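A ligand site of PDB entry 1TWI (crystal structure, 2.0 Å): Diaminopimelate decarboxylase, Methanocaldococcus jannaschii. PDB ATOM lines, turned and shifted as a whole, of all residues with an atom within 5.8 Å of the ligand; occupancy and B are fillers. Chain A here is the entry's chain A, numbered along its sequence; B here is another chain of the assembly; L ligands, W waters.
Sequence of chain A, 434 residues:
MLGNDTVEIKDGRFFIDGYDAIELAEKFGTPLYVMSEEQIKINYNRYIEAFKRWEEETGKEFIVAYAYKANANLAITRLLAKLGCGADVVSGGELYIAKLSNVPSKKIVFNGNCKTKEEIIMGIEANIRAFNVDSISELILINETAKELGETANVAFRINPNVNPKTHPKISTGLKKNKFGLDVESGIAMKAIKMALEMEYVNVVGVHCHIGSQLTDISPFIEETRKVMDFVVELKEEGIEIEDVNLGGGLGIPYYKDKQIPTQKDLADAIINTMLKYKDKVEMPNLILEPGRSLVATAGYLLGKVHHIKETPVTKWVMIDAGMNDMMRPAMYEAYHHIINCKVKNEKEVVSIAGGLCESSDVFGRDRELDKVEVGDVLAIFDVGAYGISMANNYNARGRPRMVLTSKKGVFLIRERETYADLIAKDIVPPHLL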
ATOM      1  N   ALA A  67      18.752 -14.443   7.872  1.00  0.00           N
ATOM      2  CA  ALA A  67      17.925 -13.980   8.971  1.00  0.00           C
ATOM      3  C   ALA A  67      18.789 -13.319  10.061  1.00  0.00           C
ATOM      4  O   ALA A  67      19.474 -14.016  10.858  1.00  0.00           O
ATOM      5  CB  ALA A  67      17.161 -15.130   9.566  1.00  0.00           C
ATOM      6  N   LYS A  69      18.148 -12.081  12.782  1.00  0.00           N
ATOM      7  CA  LYS A  69      17.884 -12.369  14.197  1.00  0.00           C
ATOM      8  C   LYS A  69      18.879 -13.379  14.740  1.00  0.00           C
ATOM      9  O   LYS A  69      19.081 -13.456  15.942  1.00  0.00           O
ATOM     10  CB  LYS A  69      16.448 -12.844  14.440  1.00  0.00           C
ATOM     11  CG  LYS A  69      16.108 -14.247  13.911  1.00  0.00           C
ATOM     12  CD  LYS A  69      14.691 -14.227  13.248  1.00  0.00           C
ATOM     13  CE  LYS A  69      14.879 -13.867  11.735  1.00  0.00           C
ATOM     14  NZ  LYS A  69      13.687 -13.627  10.945  1.00  0.00           N
ATOM     15  N   ALA A  70      19.493 -14.170  13.836  1.00  0.00           N
ATOM     16  CA  ALA A  70      20.479 -15.180  14.272  1.00  0.00           C
ATOM     17  C   ALA A  70      21.821 -14.611  14.748  1.00  0.00           C
ATOM     18  O   ALA A  70      22.479 -15.180  15.638  1.00  0.00           O
ATOM     19  CB  ALA A  70      20.723 -16.203  13.147  1.00  0.00           C
ATOM     20  N   ASP A  88      16.952 -10.876   5.804  1.00  0.00           N
ATOM     21  CA  ASP A  88      15.590 -11.022   6.348  1.00  0.00           C
ATOM     22  C   ASP A  88      15.683 -10.203   7.687  1.00  0.00           C
ATOM     23  O   ASP A  88      16.322 -10.646   8.619  1.00  0.00           O
ATOM     24  CB  ASP A  88      15.282 -12.500   6.632  1.00  0.00           C
ATOM     25  CG  ASP A  88      14.312 -12.685   7.783  1.00  0.00           C
ATOM     26  OD1 ASP A  88      13.485 -11.728   8.069  1.00  0.00           O
ATOM     27  OD2 ASP A  88      14.382 -13.729   8.450  1.00  0.00           O
ATOM     28  N   VAL A  90      13.735  -8.158  11.012  1.00  0.00           N
ATOM     29  CA  VAL A  90      12.441  -8.245  11.718  1.00  0.00           C
ATOM     30  C   VAL A  90      12.160  -7.034  12.598  1.00  0.00           C
ATOM     31  O   VAL A  90      11.212  -7.006  13.367  1.00  0.00           O
ATOM     32  CB  VAL A  90      12.370  -9.546  12.581  1.00  0.00           C
ATOM     33  CG1 VAL A  90      12.371 -10.753  11.697  1.00  0.00           C
ATOM     34  CG2 VAL A  90      13.503  -9.626  13.534  1.00  0.00           C
ATOM     35  N   ASN A 111      10.150  -8.967   7.879  1.00  0.00           N
ATOM     36  CA  ASN A 111       9.157  -9.827   8.558  1.00  0.00           C
ATOM     37  C   ASN A 111       8.802  -9.230   9.904  1.00  0.00           C
ATOM     38  O   ASN A 111       9.565  -8.411  10.430  1.00  0.00           O
ATOM     39  CB  ASN A 111       9.785 -11.223   8.865  1.00  0.00           C
ATOM     40  CG  ASN A 111       9.805 -12.092   7.666  1.00  0.00           C
ATOM     41  OD1 ASN A 111       8.761 -12.381   7.129  1.00  0.00           O
ATOM     42  ND2 ASN A 111      11.008 -12.535   7.216  1.00  0.00           N
ATOM     43  N   ARG A 158       2.732 -13.101   4.332  1.00  0.00           N
ATOM     44  CA  ARG A 158       3.181 -14.304   5.057  1.00  0.00           C
ATOM     45  C   ARG A 158       1.912 -15.130   5.278  1.00  0.00           C
ATOM     46  O   ARG A 158       0.996 -14.691   5.966  1.00  0.00           O
ATOM     47  CB  ARG A 158       3.789 -13.955   6.426  1.00  0.00           C
ATOM     48  CG  ARG A 158       4.147 -15.196   7.234  1.00  0.00           C
ATOM     49  CD  ARG A 158       4.910 -14.859   8.536  1.00  0.00           C
ATOM     50  NE  ARG A 158       5.393 -16.097   9.183  1.00  0.00           N
ATOM     51  CZ  ARG A 158       6.228 -16.129  10.200  1.00  0.00           C
ATOM     52  NH1 ARG A 158       6.678 -15.000  10.737  1.00  0.00           N
ATOM     53  NH2 ARG A 158       6.616 -17.307  10.696  1.00  0.00           N
ATOM     54  N   HIS A 208       5.046 -15.505   1.369  1.00  0.00           N
ATOM     55  CA  HIS A 208       6.145 -15.927   2.254  1.00  0.00           C
ATOM     56  C   HIS A 208       5.566 -16.951   3.222  1.00  0.00           C
ATOM     57  O   HIS A 208       4.348 -16.962   3.535  1.00  0.00           O
ATOM     58  CB  HIS A 208       6.632 -14.690   3.028  1.00  0.00           C
ATOM     59  CG  HIS A 208       7.486 -15.008   4.222  1.00  0.00           C
ATOM     60  ND1 HIS A 208       6.978 -15.091   5.501  1.00  0.00           N
ATOM     61  CD2 HIS A 208       8.810 -15.241   4.331  1.00  0.00           C
ATOM     62  CE1 HIS A 208       7.962 -15.350   6.348  1.00  0.00           C
ATOM     63  NE2 HIS A 208       9.091 -15.442   5.660  1.00  0.00           N
ATOM     64  N   HIS A 210       7.193 -19.392   6.734  1.00  0.00           N
ATOM     65  CA  HIS A 210       8.316 -19.804   7.534  1.00  0.00           C
ATOM     66  C   HIS A 210       7.661 -20.727   8.533  1.00  0.00           C
ATOM     67  O   HIS A 210       6.709 -20.334   9.272  1.00  0.00           O
ATOM     68  CB  HIS A 210       8.932 -18.640   8.278  1.00  0.00           C
ATOM     69  CG  HIS A 210       9.952 -19.081   9.262  1.00  0.00           C
ATOM     70  ND1 HIS A 210      11.193 -19.552   8.860  1.00  0.00           N
ATOM     71  CD2 HIS A 210       9.904 -19.212  10.610  1.00  0.00           C
ATOM     72  CE1 HIS A 210      11.860 -19.952   9.932  1.00  0.00           C
ATOM     73  NE2 HIS A 210      11.093 -19.751  11.005  1.00  0.00           N
ATOM     74  N   GLY A 212       9.282 -23.032  11.015  1.00  0.00           N
ATOM     75  CA  GLY A 212       9.823 -23.529  12.277  1.00  0.00           C
ATOM     76  C   GLY A 212      11.330 -23.425  12.205  1.00  0.00           C
ATOM     77  O   GLY A 212      11.859 -22.829  11.246  1.00  0.00           O
ATOM     78  N   SER A 213      12.029 -24.025  13.164  1.00  0.00           N
ATOM     79  CA  SER A 213      13.485 -23.894  13.213  1.00  0.00           C
ATOM     80  C   SER A 213      14.133 -25.179  13.732  1.00  0.00           C
ATOM     81  O   SER A 213      13.482 -25.971  14.436  1.00  0.00           O
ATOM     82  CB  SER A 213      13.847 -22.695  14.127  1.00  0.00           C
ATOM     83  OG  SER A 213      15.233 -22.288  14.036  1.00  0.00           O
ATOM     84  N   GLN A 214      15.383 -25.364  13.348  1.00  0.00           N
ATOM     85  CA  GLN A 214      16.186 -26.541  13.678  1.00  0.00           C
ATOM     86  C   GLN A 214      15.415 -27.798  13.277  1.00  0.00           C
ATOM     87  O   GLN A 214      15.239 -28.739  14.073  1.00  0.00           O
ATOM     88  CB  GLN A 214      16.562 -26.519  15.185  1.00  0.00           C
ATOM     89  CG  GLN A 214      17.377 -27.728  15.665  1.00  0.00           C
ATOM     90  CD  GLN A 214      18.680 -27.959  14.869  1.00  0.00           C
ATOM     91  OE1 GLN A 214      19.256 -29.088  14.861  1.00  0.00           O
ATOM     92  NE2 GLN A 214      19.158 -26.919  14.208  1.00  0.00           N
ATOM     93  N   GLY A 248      11.091 -18.976   3.593  1.00  0.00           N
ATOM     94  CA  GLY A 248      11.537 -18.890   4.997  1.00  0.00           C
ATOM     95  C   GLY A 248      12.836 -19.630   5.292  1.00  0.00           C
ATOM     96  O   GLY A 248      13.607 -19.984   4.384  1.00  0.00           O
ATOM     97  N   GLY A 249      13.096 -19.856   6.573  1.00  0.00           N
ATOM     98  CA  GLY A 249      14.315 -20.553   6.926  1.00  0.00           C
ATOM     99  C   GLY A 249      13.968 -21.833   7.695  1.00  0.00           C
ATOM    100  O   GLY A 249      12.943 -22.519   7.391  1.00  0.00           O
ATOM    101  N   GLY A 250      14.815 -22.184   8.643  1.00  0.00           N
ATOM    102  CA  GLY A 250      14.547 -23.331   9.478  1.00  0.00           C
ATOM    103  C   GLY A 250      15.420 -24.570   9.266  1.00  0.00           C
ATOM    104  O   GLY A 250      15.278 -25.488  10.082  1.00  0.00           O
ATOM    105  N   LEU A 251      16.254 -24.643   8.206  1.00  0.00           N
ATOM    106  CA  LEU A 251      17.098 -25.871   8.071  1.00  0.00           C
ATOM    107  C   LEU A 251      17.936 -26.092   9.359  1.00  0.00           C
ATOM    108  O   LEU A 251      18.625 -25.184   9.824  1.00  0.00           O
ATOM    109  CB  LEU A 251      18.089 -25.766   6.885  1.00  0.00           C
ATOM    110  CG  LEU A 251      18.871 -27.060   6.591  1.00  0.00           C
ATOM    111  CD1 LEU A 251      17.838 -28.146   6.136  1.00  0.00           C
ATOM    112  CD2 LEU A 251      19.884 -26.822   5.389  1.00  0.00           C
ATOM    113  N   GLU A 290      15.281 -17.884   3.768  1.00  0.00           N
ATOM    114  CA  GLU A 290      15.711 -17.017   4.882  1.00  0.00           C
ATOM    115  C   GLU A 290      16.491 -17.781   5.906  1.00  0.00           C
ATOM    116  O   GLU A 290      16.175 -17.747   7.074  1.00  0.00           O
ATOM    117  CB  GLU A 290      14.480 -16.381   5.574  1.00  0.00           C
ATOM    118  CG  GLU A 290      13.604 -15.482   4.629  1.00  0.00           C
ATOM    119  CD  GLU A 290      12.280 -15.006   5.313  1.00  0.00           C
ATOM    120  OE1 GLU A 290      11.769 -15.679   6.246  1.00  0.00           O
ATOM    121  OE2 GLU A 290      11.743 -13.973   4.881  1.00  0.00           O
ATOM    122  N   PRO A 291      17.563 -18.496   5.478  1.00  0.00           N
ATOM    123  CA  PRO A 291      18.296 -19.233   6.497  1.00  0.00           C
ATOM    124  C   PRO A 291      18.959 -18.299   7.522  1.00  0.00           C
ATOM    125  O   PRO A 291      19.437 -17.199   7.150  1.00  0.00           O
ATOM    126  CB  PRO A 291      19.333 -20.023   5.684  1.00  0.00           C
ATOM    127  CG  PRO A 291      19.666 -19.075   4.529  1.00  0.00           C
ATOM    128  CD  PRO A 291      18.265 -18.471   4.175  1.00  0.00           C
ATOM    129  N   GLY A 292      18.977 -18.740   8.787  1.00  0.00           N
ATOM    130  CA  GLY A 292      19.637 -17.996   9.850  1.00  0.00           C
ATOM    131  C   GLY A 292      20.710 -18.941  10.428  1.00  0.00           C
ATOM    132  O   GLY A 292      21.903 -18.867  10.091  1.00  0.00           O
ATOM    133  N   ARG A 293      20.258 -19.846  11.284  1.00  0.00           N
ATOM    134  CA  ARG A 293      21.109 -20.837  11.946  1.00  0.00           C
ATOM    135  C   ARG A 293      21.982 -21.550  10.933  1.00  0.00           C
ATOM    136  O   ARG A 293      23.181 -21.674  11.147  1.00  0.00           O
ATOM    137  CB  ARG A 293      20.225 -21.853  12.660  1.00  0.00           C
ATOM    138  CG  ARG A 293      20.919 -22.678  13.763  1.00  0.00           C
ATOM    139  CD  ARG A 293      19.973 -23.875  14.153  1.00  0.00           C
ATOM    140  NE  ARG A 293      18.644 -23.403  14.562  1.00  0.00           N
ATOM    141  CZ  ARG A 293      18.340 -22.998  15.806  1.00  0.00           C
ATOM    142  NH1 ARG A 293      19.245 -23.025  16.801  1.00  0.00           N
ATOM    143  NH2 ARG A 293      17.137 -22.512  16.019  1.00  0.00           N
ATOM    144  N   SER A 294      21.420 -22.000   9.804  1.00  0.00           N
ATOM    145  CA  SER A 294      22.261 -22.744   8.871  1.00  0.00           C
ATOM    146  C   SER A 294      23.344 -21.943   8.108  1.00  0.00           C
ATOM    147  O   SER A 294      24.145 -22.536   7.343  1.00  0.00           O
ATOM    148  CB  SER A 294      21.384 -23.575   7.884  1.00  0.00           C
ATOM    149  OG  SER A 294      20.512 -22.744   7.142  1.00  0.00           O
ATOM    150  N   TYR A 387      21.959 -17.374  17.534  1.00  0.00           N
ATOM    151  CA  TYR A 387      21.202 -17.250  18.782  1.00  0.00           C
ATOM    152  C   TYR A 387      22.175 -17.434  19.910  1.00  0.00           C
ATOM    153  O   TYR A 387      21.902 -18.115  20.885  1.00  0.00           O
ATOM    154  CB  TYR A 387      20.109 -18.305  18.838  1.00  0.00           C
ATOM    155  CG  TYR A 387      19.270 -18.245  17.557  1.00  0.00           C
ATOM    156  CD1 TYR A 387      18.432 -17.178  17.319  1.00  0.00           C
ATOM    157  CD2 TYR A 387      19.423 -19.201  16.566  1.00  0.00           C
ATOM    158  CE1 TYR A 387      17.722 -17.053  16.072  1.00  0.00           C
ATOM    159  CE2 TYR A 387      18.755 -19.127  15.341  1.00  0.00           C
ATOM    160  CZ  TYR A 387      17.899 -18.038  15.094  1.00  0.00           C
ATOM    161  OH  TYR A 387      17.243 -17.963  13.881  1.00  0.00           O
ATOM    162  N   CYS B 358      10.213 -12.226  16.248  1.00  0.00           N
ATOM    163  CA  CYS B 358       9.892 -13.372  15.409  1.00  0.00           C
ATOM    164  C   CYS B 358      10.201 -14.701  16.013  1.00  0.00           C
ATOM    165  O   CYS B 358      10.834 -15.541  15.362  1.00  0.00           O
ATOM    166  CB  CYS B 358      10.581 -13.238  14.038  1.00  0.00           C
ATOM    167  SG  CYS B 358       9.368 -12.696  12.715  1.00  0.00           S
ATOM    168  N   GLU B 359       9.790 -14.861  17.279  1.00  0.00           N
ATOM    169  CA  GLU B 359       9.936 -16.053  18.122  1.00  0.00           C
ATOM    170  C   GLU B 359       8.527 -16.379  18.555  1.00  0.00           C
ATOM    171  O   GLU B 359       7.778 -15.514  19.106  1.00  0.00           O
ATOM    172  CB  GLU B 359      10.650 -15.766  19.432  1.00  0.00           C
ATOM    173  CG  GLU B 359      12.079 -15.819  19.418  1.00  0.00           C
ATOM    174  CD  GLU B 359      12.583 -17.170  19.042  1.00  0.00           C
ATOM    175  OE1 GLU B 359      13.501 -17.178  18.251  1.00  0.00           O
ATOM    176  OE2 GLU B 359      12.063 -18.189  19.520  1.00  0.00           O
ATOM    177  N   TYR B 395      17.720  -9.026  21.651  1.00  0.00           N
ATOM    178  CA  TYR B 395      17.251  -9.966  20.627  1.00  0.00           C
ATOM    179  C   TYR B 395      16.312  -9.272  19.610  1.00  0.00           C
ATOM    180  O   TYR B 395      15.464  -8.426  19.991  1.00  0.00           O
ATOM    181  CB  TYR B 395      16.581 -11.129  21.327  1.00  0.00           C
ATOM    182  CG  TYR B 395      16.237 -12.266  20.428  1.00  0.00           C
ATOM    183  CD1 TYR B 395      17.165 -12.806  19.551  1.00  0.00           C
ATOM    184  CD2 TYR B 395      14.977 -12.871  20.517  1.00  0.00           C
ATOM    185  CE1 TYR B 395      16.845 -13.946  18.784  1.00  0.00           C
ATOM    186  CE2 TYR B 395      14.665 -13.988  19.756  1.00  0.00           C
ATOM    187  CZ  TYR B 395      15.615 -14.504  18.895  1.00  0.00           C
ATOM    188  OH  TYR B 395      15.276 -15.587  18.139  1.00  0.00           O
HETATM  189  N1  LIG L   1      12.454 -16.422   8.712  1.00  0.00           N
HETATM  190  C1  LIG L   1      11.601 -16.112   9.759  1.00  0.00           C
HETATM  191  C2  LIG L   1      10.263 -15.428   9.379  1.00  0.00           C
HETATM  192  C3  LIG L   1      12.033 -16.414  11.048  1.00  0.00           C
HETATM  193  O1  LIG L   1      11.174 -16.101  12.050  1.00  0.00           O
HETATM  194  C4  LIG L   1      13.222 -17.047  11.324  1.00  0.00           C
HETATM  195  C5  LIG L   1      13.601 -17.342  12.815  1.00  0.00           C
HETATM  196  O2  LIG L   1      12.950 -16.789  13.649  1.00  0.00           O
HETATM  197  C6  LIG L   1      14.100 -17.358  10.261  1.00  0.00           C
HETATM  198  C7  LIG L   1      13.666 -17.053   8.981  1.00  0.00           C
HETATM  199  C8  LIG L   1      15.447 -18.048  10.368  1.00  0.00           C
HETATM  200  O3  LIG L   1      15.347 -19.351  11.004  1.00  0.00           O
HETATM  201  P1  LIG L   1      16.595 -20.325  11.110  1.00  0.00           P
HETATM  202  O4  LIG L   1      16.067 -21.490  11.823  1.00  0.00           O
HETATM  203  O5  LIG L   1      17.607 -19.569  11.930  1.00  0.00           O
HETATM  204  O6  LIG L   1      17.051 -20.642   9.757  1.00  0.00           O
HETATM  205  O   HOH W   1      17.260 -23.830  12.008  1.00  0.00           O
HETATM  206  O   HOH W   2      18.778 -22.365   9.083  1.00  0.00           O
HETATM  207  O   HOH W   3       8.583 -16.302  12.644  1.00  0.00           O
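The side-chain hydroxyl (OG) of Ser 213 sits at hydrogen-bond distance from an oxygen (O4) of the ligand (2.5 Å).
OH of Tyr 387 is in hydrogen-bond range of O5 of the ligand.
N1 of the ligand sits at hydrogen-bond distance from OE1 of Glu 290.
The backbone NH of Arg 293 lies within hydrogen-bond range of an oxygen (O5) of the ligand, 2.7 Å away.
N of Gly 292 lies within hydrogen-bond range of O6 of the ligand (2.9 Å).
An oxygen (O6) of the ligand is in hydrogen-bond range of the backbone NH (N) of Gly 250, at 2.9 Å.
O of Cys 358 of chain B sits at hydrogen-bond distance from O1 of the ligand (3.4 Å).
A ring nitrogen (ND1) of His 210 is in hydrogen-bond range of a nitrogen (N1) of the ligand.
OD2 of Asp 88 lies close to N1 of the ligand, 3.3 Å away.
CB of Ala 67 touches C8 of the ligand, 3.5 Å away.
Lys 69 touches the ligand.
Asn 111 touches the ligand.
NH1 of Arg 158 touches C2 of the ligand (3.9 Å).
His 208 touches the ligand (CE1 to C2, 3.8 Å).
N of Gly 249 touches C7 of the ligand, at 3.7 Å.
Pro 291 touches the ligand.
Hydrophobic or aromatic side chains within 4 Å of the ligand: Ala 67, His 208, His 210 and Tyr 387.
The guanidinium group (NH2) of Arg 293 sits at hydrogen-bond distance from the side-chain hydroxyl (OG) of Ser 213 (2.8 Å).
The backbone NH (N) of Glu 290 sits at hydrogen-bond distance from the backbone carbonyl oxygen (O) of Gly 248.
O of Gly 250 is in hydrogen-bond range of N of Gln 214, 3.3 Å away.
OD1 of Asp 88 sits at hydrogen-bond distance from ND2 of Asn 111 (2.7 Å).
A ring nitrogen (ND1) of His 210 lies within hydrogen-bond range of the backbone NH of Gly 249 (3.0 Å).
O of His 210 sits at hydrogen-bond distance from NH2 of Arg 158.
N of Ala 67 sits at hydrogen-bond distance from O of Pro 291 (2.9 Å).
The side-chain amide oxygen (OD1) of Asn 111 lies close to a ring nitrogen (NE2) of His 208 (3.4 Å).
Water W2 lies within hydrogen-bond range of O6 of the ligand (2.5 Å), OG of Ser 294 (2.6 Å) and O of Leu 251 (2.9 Å).
Water W1 lies within hydrogen-bond range of an oxygen (O4) of the ligand (2.6 Å), the backbone NH (N) of Gln 214 (2.8 Å), the backbone carbonyl oxygen (O) of Leu 251 (2.9 Å), the guanidinium group (NE) of Arg 293 (2.9 Å), the backbone carbonyl oxygen (O) of Gly 250 (3.2 Å) and the side-chain hydroxyl (OG) of Ser 213 (3.3 Å).
Water W3 lies within hydrogen-bond range of an oxygen (O1) of the ligand (2.7 Å), the guanidinium group (NH2) of Arg 158 (2.9 Å) and the side-chain sulfur (SG) of Cys 358 of chain B (3.7 Å).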
